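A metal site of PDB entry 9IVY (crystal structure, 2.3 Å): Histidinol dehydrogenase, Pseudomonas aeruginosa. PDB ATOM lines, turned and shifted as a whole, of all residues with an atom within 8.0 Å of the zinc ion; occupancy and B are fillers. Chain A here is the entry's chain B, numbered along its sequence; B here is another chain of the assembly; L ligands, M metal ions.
OE1 of Glu 363 lies within hydrogen-bond range of NE2 of Gln 265, 3.1 Å away.
NE2 of His 426 of chain B sits close to O of Ser 264, at 3.4 Å.
The side-chain carboxylate (OE2) of Glu 267 is in hydrogen-bond range of a ring nitrogen (ND1) of His 426 of chain B, 2.5 Å away.
A ring nitrogen (ND1) of His 268 sits at hydrogen-bond distance from the side-chain hydroxyl (OH) of Tyr 144 (2.8 Å).
ND1 of His 268 sits close to O13 of the ligand (3.4 Å).
An oxygen (O13) of the ligand sits at hydrogen-bond distance from the side-chain hydroxyl (OG) of Ser 243, at 2.6 Å.
The zinc ion is bound by OE2 of Glu 363.
OD2 of Asp 367 is bound to the zinc ion (1.9 Å).
NE2 of His 426 of chain B binds the zinc ion, at 2.3 Å.
NE2 of His 268 is bound to the zinc ion, 2.3 Å away.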
ATOM      1  N   TYR A 144     -16.839 -12.298 -18.851  1.00  0.00           N
ATOM      2  CA  TYR A 144     -16.885 -13.490 -19.698  1.00  0.00           C
ATOM      3  C   TYR A 144     -18.150 -14.292 -19.420  1.00  0.00           C
ATOM      4  O   TYR A 144     -18.121 -15.295 -18.700  1.00  0.00           O
ATOM      5  CB  TYR A 144     -15.633 -14.339 -19.487  1.00  0.00           C
ATOM      6  CG  TYR A 144     -14.366 -13.552 -19.714  1.00  0.00           C
ATOM      7  CD1 TYR A 144     -13.900 -13.305 -20.994  1.00  0.00           C
ATOM      8  CD2 TYR A 144     -13.650 -13.029 -18.645  1.00  0.00           C
ATOM      9  CE1 TYR A 144     -12.758 -12.569 -21.208  1.00  0.00           C
ATOM     10  CE2 TYR A 144     -12.500 -12.290 -18.848  1.00  0.00           C
ATOM     11  CZ  TYR A 144     -12.048 -12.067 -20.136  1.00  0.00           C
ATOM     12  OH  TYR A 144     -10.907 -11.339 -20.365  1.00  0.00           O
ATOM     13  N   SER A 243      -2.830 -16.776 -21.200  1.00  0.00           N
ATOM     14  CA  SER A 243      -3.610 -16.399 -22.366  1.00  0.00           C
ATOM     15  C   SER A 243      -2.708 -16.200 -23.575  1.00  0.00           C
ATOM     16  O   SER A 243      -1.793 -15.378 -23.552  1.00  0.00           O
ATOM     17  CB  SER A 243      -4.390 -15.118 -22.058  1.00  0.00           C
ATOM     18  OG  SER A 243      -5.629 -15.094 -22.738  1.00  0.00           O
ATOM     19  N   GLU A 244      -2.967 -16.953 -24.643  1.00  0.00           N
ATOM     20  CA  GLU A 244      -2.129 -16.867 -25.825  1.00  0.00           C
ATOM     21  C   GLU A 244      -2.941 -17.200 -27.067  1.00  0.00           C
ATOM     22  O   GLU A 244      -3.968 -17.889 -26.997  1.00  0.00           O
ATOM     23  CB  GLU A 244      -0.907 -17.788 -25.714  1.00  0.00           C
ATOM     24  CG  GLU A 244      -1.209 -19.230 -25.284  1.00  0.00           C
ATOM     25  CD  GLU A 244      -2.045 -19.987 -26.295  1.00  0.00           C
ATOM     26  OE1 GLU A 244      -3.181 -20.382 -25.950  1.00  0.00           O
ATOM     27  OE2 GLU A 244      -1.585 -20.142 -27.450  1.00  0.00           O
ATOM     28  N   ASP A 261      -7.814 -10.662 -35.364  1.00  0.00           N
ATOM     29  CA  ASP A 261      -7.704 -11.911 -34.616  1.00  0.00           C
ATOM     30  C   ASP A 261      -6.631 -11.810 -33.546  1.00  0.00           C
ATOM     31  O   ASP A 261      -6.822 -12.258 -32.414  1.00  0.00           O
ATOM     32  CB  ASP A 261      -7.417 -13.090 -35.558  1.00  0.00           C
ATOM     33  CG  ASP A 261      -8.589 -13.406 -36.471  1.00  0.00           C
ATOM     34  OD1 ASP A 261      -9.688 -12.873 -36.238  1.00  0.00           O
ATOM     35  OD2 ASP A 261      -8.398 -14.188 -37.439  1.00  0.00           O
ATOM     36  N   PHE A 263      -5.641  -8.896 -32.304  1.00  0.00           N
ATOM     37  CA  PHE A 263      -6.202  -7.924 -31.371  1.00  0.00           C
ATOM     38  C   PHE A 263      -7.098  -8.599 -30.346  1.00  0.00           C
ATOM     39  O   PHE A 263      -7.071  -8.248 -29.155  1.00  0.00           O
ATOM     40  CB  PHE A 263      -6.999  -6.859 -32.125  1.00  0.00           C
ATOM     41  CG  PHE A 263      -6.163  -5.741 -32.672  1.00  0.00           C
ATOM     42  CD1 PHE A 263      -4.787  -5.788 -32.592  1.00  0.00           C
ATOM     43  CD2 PHE A 263      -6.764  -4.636 -33.257  1.00  0.00           C
ATOM     44  CE1 PHE A 263      -4.018  -4.751 -33.094  1.00  0.00           C
ATOM     45  CE2 PHE A 263      -6.003  -3.596 -33.754  1.00  0.00           C
ATOM     46  CZ  PHE A 263      -4.623  -3.655 -33.682  1.00  0.00           C
ATOM     47  N   SER A 264      -7.906  -9.579 -30.775  1.00  0.00           N
ATOM     48  CA  SER A 264      -8.900 -10.177 -29.897  1.00  0.00           C
ATOM     49  C   SER A 264      -8.240 -10.884 -28.714  1.00  0.00           C
ATOM     50  O   SER A 264      -8.709 -10.752 -27.580  1.00  0.00           O
ATOM     51  CB  SER A 264      -9.790 -11.133 -30.691  1.00  0.00           C
ATOM     52  OG  SER A 264      -9.291 -12.458 -30.664  1.00  0.00           O
ATOM     53  N   GLN A 265      -7.165 -11.615 -28.959  1.00  0.00           N
ATOM     54  CA  GLN A 265      -6.431 -12.182 -27.828  1.00  0.00           C
ATOM     55  C   GLN A 265      -5.737 -11.087 -27.036  1.00  0.00           C
ATOM     56  O   GLN A 265      -5.643 -11.169 -25.803  1.00  0.00           O
ATOM     57  CB  GLN A 265      -5.421 -13.221 -28.319  1.00  0.00           C
ATOM     58  CG  GLN A 265      -4.306 -13.545 -27.349  1.00  0.00           C
ATOM     59  CD  GLN A 265      -4.788 -14.244 -26.086  1.00  0.00           C
ATOM     60  OE1 GLN A 265      -4.264 -14.005 -25.005  1.00  0.00           O
ATOM     61  NE2 GLN A 265      -5.797 -15.098 -26.220  1.00  0.00           N
ATOM     62  N   ALA A 266      -5.257 -10.042 -27.728  1.00  0.00           N
ATOM     63  CA  ALA A 266      -4.505  -8.980 -27.062  1.00  0.00           C
ATOM     64  C   ALA A 266      -5.383  -8.146 -26.131  1.00  0.00           C
ATOM     65  O   ALA A 266      -4.885  -7.646 -25.117  1.00  0.00           O
ATOM     66  CB  ALA A 266      -3.845  -8.078 -28.110  1.00  0.00           C
ATOM     67  N   GLU A 267      -6.666  -7.972 -26.460  1.00  0.00           N
ATOM     68  CA  GLU A 267      -7.547  -7.151 -25.644  1.00  0.00           C
ATOM     69  C   GLU A 267      -7.970  -7.824 -24.343  1.00  0.00           C
ATOM     70  O   GLU A 267      -8.630  -7.180 -23.520  1.00  0.00           O
ATOM     71  CB  GLU A 267      -8.781  -6.737 -26.444  1.00  0.00           C
ATOM     72  CG  GLU A 267      -9.919  -7.751 -26.465  1.00  0.00           C
ATOM     73  CD  GLU A 267     -11.082  -7.299 -27.334  1.00  0.00           C
ATOM     74  OE1 GLU A 267     -11.175  -6.088 -27.615  1.00  0.00           O
ATOM     75  OE2 GLU A 267     -11.902  -8.152 -27.764  1.00  0.00           O
ATOM     76  N   HIS A 268      -7.583  -9.086 -24.139  1.00  0.00           N
ATOM     77  CA  HIS A 268      -7.929  -9.786 -22.896  1.00  0.00           C
ATOM     78  C   HIS A 268      -7.312  -9.103 -21.689  1.00  0.00           C
ATOM     79  O   HIS A 268      -8.016  -8.666 -20.765  1.00  0.00           O
ATOM     80  CB  HIS A 268      -7.455 -11.232 -22.972  1.00  0.00           C
ATOM     81  CG  HIS A 268      -8.517 -12.203 -23.376  1.00  0.00           C
ATOM     82  ND1 HIS A 268      -9.655 -12.416 -22.631  1.00  0.00           N
ATOM     83  CD2 HIS A 268      -8.609 -13.043 -24.439  1.00  0.00           C
ATOM     84  CE1 HIS A 268     -10.411 -13.332 -23.217  1.00  0.00           C
ATOM     85  NE2 HIS A 268      -9.788 -13.730 -24.316  1.00  0.00           N
ATOM     86  N   HIS A 334      -3.791 -22.645 -28.053  1.00  0.00           N
ATOM     87  CA  HIS A 334      -4.749 -22.285 -29.093  1.00  0.00           C
ATOM     88  C   HIS A 334      -3.970 -21.939 -30.354  1.00  0.00           C
ATOM     89  O   HIS A 334      -3.144 -21.016 -30.336  1.00  0.00           O
ATOM     90  CB  HIS A 334      -5.625 -21.113 -28.670  1.00  0.00           C
ATOM     91  CG  HIS A 334      -6.444 -21.377 -27.446  1.00  0.00           C
ATOM     92  ND1 HIS A 334      -5.898 -21.352 -26.174  1.00  0.00           N
ATOM     93  CD2 HIS A 334      -7.747 -21.682 -27.285  1.00  0.00           C
ATOM     94  CE1 HIS A 334      -6.836 -21.626 -25.291  1.00  0.00           C
ATOM     95  NE2 HIS A 334      -7.971 -21.826 -25.941  1.00  0.00           N
ATOM     96  N   ALA A 362     -11.829 -18.212 -35.714  1.00  0.00           N
ATOM     97  CA  ALA A 362     -10.888 -17.507 -34.858  1.00  0.00           C
ATOM     98  C   ALA A 362     -11.277 -17.720 -33.398  1.00  0.00           C
ATOM     99  O   ALA A 362     -12.283 -18.382 -33.093  1.00  0.00           O
ATOM    100  CB  ALA A 362     -10.832 -16.014 -35.219  1.00  0.00           C
ATOM    101  N   GLU A 363     -10.474 -17.150 -32.498  1.00  0.00           N
ATOM    102  CA  GLU A 363     -10.658 -17.368 -31.065  1.00  0.00           C
ATOM    103  C   GLU A 363     -12.022 -16.882 -30.589  1.00  0.00           C
ATOM    104  O   GLU A 363     -12.629 -17.494 -29.699  1.00  0.00           O
ATOM    105  CB  GLU A 363      -9.536 -16.685 -30.284  1.00  0.00           C
ATOM    106  CG  GLU A 363      -9.994 -15.950 -29.038  1.00  0.00           C
ATOM    107  CD  GLU A 363      -8.853 -15.322 -28.271  1.00  0.00           C
ATOM    108  OE1 GLU A 363      -7.683 -15.546 -28.646  1.00  0.00           O
ATOM    109  OE2 GLU A 363      -9.123 -14.591 -27.297  1.00  0.00           O
ATOM    110  N   ALA A 364     -12.517 -15.782 -31.161  1.00  0.00           N
ATOM    111  CA  ALA A 364     -13.797 -15.238 -30.726  1.00  0.00           C
ATOM    112  C   ALA A 364     -14.924 -16.261 -30.864  1.00  0.00           C
ATOM    113  O   ALA A 364     -15.839 -16.279 -30.047  1.00  0.00           O
ATOM    114  CB  ALA A 364     -14.133 -13.966 -31.512  1.00  0.00           C
ATOM    115  N   LEU A 365     -14.862 -17.117 -31.891  1.00  0.00           N
ATOM    116  CA  LEU A 365     -15.850 -18.175 -32.021  1.00  0.00           C
ATOM    117  C   LEU A 365     -15.611 -19.289 -31.014  1.00  0.00           C
ATOM    118  O   LEU A 365     -16.558 -19.820 -30.421  1.00  0.00           O
ATOM    119  CB  LEU A 365     -15.853 -18.722 -33.447  1.00  0.00           C
ATOM    120  CG  LEU A 365     -16.254 -17.729 -34.537  1.00  0.00           C
ATOM    121  CD1 LEU A 365     -16.595 -18.465 -35.827  1.00  0.00           C
ATOM    122  CD2 LEU A 365     -17.429 -16.878 -34.090  1.00  0.00           C
ATOM    123  N   GLY A 366     -14.344 -19.650 -30.790  1.00  0.00           N
ATOM    124  CA  GLY A 366     -14.049 -20.608 -29.734  1.00  0.00           C
ATOM    125  C   GLY A 366     -14.447 -20.097 -28.367  1.00  0.00           C
ATOM    126  O   GLY A 366     -14.979 -20.851 -27.547  1.00  0.00           O
ATOM    127  N   ASP A 367     -14.231 -18.808 -28.106  1.00  0.00           N
ATOM    128  CA  ASP A 367     -14.531 -18.241 -26.797  1.00  0.00           C
ATOM    129  C   ASP A 367     -16.010 -18.335 -26.475  1.00  0.00           C
ATOM    130  O   ASP A 367     -16.405 -18.738 -25.380  1.00  0.00           O
ATOM    131  CB  ASP A 367     -14.068 -16.785 -26.743  1.00  0.00           C
ATOM    132  CG  ASP A 367     -12.611 -16.632 -26.324  1.00  0.00           C
ATOM    133  OD1 ASP A 367     -11.848 -17.617 -26.430  1.00  0.00           O
ATOM    134  OD2 ASP A 367     -12.235 -15.536 -25.883  1.00  0.00           O
ATOM    135  N   TYR A 368     -16.862 -17.965 -27.433  1.00  0.00           N
ATOM    136  CA  TYR A 368     -18.279 -17.766 -27.137  1.00  0.00           C
ATOM    137  C   TYR A 368     -19.169 -18.940 -27.515  1.00  0.00           C
ATOM    138  O   TYR A 368     -20.299 -19.025 -27.019  1.00  0.00           O
ATOM    139  CB  TYR A 368     -18.787 -16.510 -27.849  1.00  0.00           C
ATOM    140  CG  TYR A 368     -18.246 -15.232 -27.259  1.00  0.00           C
ATOM    141  CD1 TYR A 368     -18.810 -14.683 -26.103  1.00  0.00           C
ATOM    142  CD2 TYR A 368     -17.148 -14.583 -27.826  1.00  0.00           C
ATOM    143  CE1 TYR A 368     -18.304 -13.528 -25.551  1.00  0.00           C
ATOM    144  CE2 TYR A 368     -16.645 -13.423 -27.282  1.00  0.00           C
ATOM    145  CZ  TYR A 368     -17.227 -12.894 -26.143  1.00  0.00           C
ATOM    146  OH  TYR A 368     -16.734 -11.744 -25.588  1.00  0.00           O
ATOM    147  N   LEU B 423     -15.788  -6.088 -25.676  1.00  0.00           N
ATOM    148  CA  LEU B 423     -14.638  -6.810 -26.225  1.00  0.00           C
ATOM    149  C   LEU B 423     -14.676  -6.664 -27.749  1.00  0.00           C
ATOM    150  O   LEU B 423     -14.942  -7.611 -28.507  1.00  0.00           O
ATOM    151  CB  LEU B 423     -14.647  -8.261 -25.777  1.00  0.00           C
ATOM    152  CG  LEU B 423     -14.269  -8.432 -24.311  1.00  0.00           C
ATOM    153  CD1 LEU B 423     -14.828  -9.722 -23.730  1.00  0.00           C
ATOM    154  CD2 LEU B 423     -12.761  -8.365 -24.153  1.00  0.00           C
ATOM    155  N   HIS B 426     -12.778  -8.914 -30.306  1.00  0.00           N
ATOM    156  CA  HIS B 426     -13.509 -10.161 -30.464  1.00  0.00           C
ATOM    157  C   HIS B 426     -14.669 -10.006 -31.420  1.00  0.00           C
ATOM    158  O   HIS B 426     -14.865 -10.819 -32.329  1.00  0.00           O
ATOM    159  CB  HIS B 426     -14.033 -10.648 -29.106  1.00  0.00           C
ATOM    160  CG  HIS B 426     -12.984 -11.248 -28.244  1.00  0.00           C
ATOM    161  ND1 HIS B 426     -12.337 -10.539 -27.264  1.00  0.00           N
ATOM    162  CD2 HIS B 426     -12.483 -12.508 -28.195  1.00  0.00           C
ATOM    163  CE1 HIS B 426     -11.459 -11.322 -26.658  1.00  0.00           C
ATOM    164  NE2 HIS B 426     -11.534 -12.524 -27.209  1.00  0.00           N
HETATM  165  P1  LIG L   1      -9.444 -12.942 -12.907  1.00  0.00           P
HETATM  166  O1  LIG L   1      -8.873 -14.182 -13.553  1.00  0.00           O
HETATM  167  O2  LIG L   1     -10.713 -13.272 -12.158  1.00  0.00           O
HETATM  168  O3  LIG L   1      -8.321 -12.334 -11.877  1.00  0.00           O
HETATM  169  C1  LIG L   1      -8.717 -11.262 -11.044  1.00  0.00           C
HETATM  170  C2  LIG L   1      -8.318 -11.639  -9.612  1.00  0.00           C
HETATM  171  O4  LIG L   1      -7.014 -11.716  -9.530  1.00  0.00           O
HETATM  172  C3  LIG L   1      -8.714 -10.523  -8.647  1.00  0.00           C
HETATM  173  O5  LIG L   1      -9.970 -10.730  -8.176  1.00  0.00           O
HETATM  174  C4  LIG L   1      -7.674 -10.650  -7.504  1.00  0.00           C
HETATM  175  O6  LIG L   1      -8.254 -11.458  -6.367  1.00  0.00           O
HETATM  176  C5  LIG L   1      -6.636 -11.247  -8.012  1.00  0.00           C
HETATM  177  N1  LIG L   1      -5.516 -10.319  -8.066  1.00  0.00           N
HETATM  178  C6  LIG L   1      -5.319  -9.258  -8.861  1.00  0.00           C
HETATM  179  N2  LIG L   1      -4.144  -8.701  -8.532  1.00  0.00           N
HETATM  180  C7  LIG L   1      -3.620  -9.422  -7.517  1.00  0.00           C
HETATM  181  C8  LIG L   1      -2.420  -9.292  -6.798  1.00  0.00           C
HETATM  182  N3  LIG L   1      -1.386  -8.363  -6.888  1.00  0.00           N
HETATM  183  N4  LIG L   1      -2.130 -10.150  -5.831  1.00  0.00           N
HETATM  184  C9  LIG L   1      -2.985 -11.157  -5.544  1.00  0.00           C
HETATM  185  N5  LIG L   1      -4.157 -11.294  -6.253  1.00  0.00           N
HETATM  186  C10 LIG L   1      -4.457 -10.416  -7.229  1.00  0.00           C
HETATM  187  O7  LIG L   1      -9.775 -11.798 -14.079  1.00  0.00           O
HETATM  188  P2  LIG L   1      -8.656 -11.254 -15.182  1.00  0.00           P
HETATM  189  O8  LIG L   1      -9.381 -10.515 -16.309  1.00  0.00           O
HETATM  190  O9  LIG L   1      -7.681 -10.337 -14.505  1.00  0.00           O
HETATM  191  O10 LIG L   1      -7.814 -12.576 -15.802  1.00  0.00           O
HETATM  192  C11 LIG L   1      -8.509 -13.479 -16.636  1.00  0.00           C
HETATM  193  C12 LIG L   1      -7.443 -14.313 -17.367  1.00  0.00           C
HETATM  194  O11 LIG L   1      -8.058 -15.678 -17.841  1.00  0.00           O
HETATM  195  C13 LIG L   1      -7.074 -13.694 -18.421  1.00  0.00           C
HETATM  196  O12 LIG L   1      -5.659 -13.905 -18.674  1.00  0.00           O
HETATM  197  C14 LIG L   1      -7.973 -14.333 -19.669  1.00  0.00           C
HETATM  198  O13 LIG L   1      -7.243 -14.188 -20.920  1.00  0.00           O
HETATM  199  C15 LIG L   1      -8.119 -15.568 -19.398  1.00  0.00           C
HETATM  200  N6  LIG L   1      -9.489 -16.063 -19.879  1.00  0.00           N
HETATM  201  C16 LIG L   1      -9.582 -17.303 -20.552  1.00  0.00           C
HETATM  202  C17 LIG L   1     -10.883 -17.736 -21.220  1.00  0.00           C
HETATM  203  C18 LIG L   1     -10.885 -19.109 -21.904  1.00  0.00           C
HETATM  204  O14 LIG L   1     -10.057 -19.910 -21.625  1.00  0.00           O
HETATM  205  N7  LIG L   1     -11.906 -19.409 -22.885  1.00  0.00           N
HETATM  206  C19 LIG L   1     -12.237 -17.181 -20.712  1.00  0.00           C
HETATM  207  C20 LIG L   1     -12.079 -15.885 -19.832  1.00  0.00           C
HETATM  208  C21 LIG L   1     -10.668 -15.261 -19.626  1.00  0.00           C
HETATM  209 ZN    ZN M   1     -10.718 -14.417 -26.277  1.00  0.00          ZN
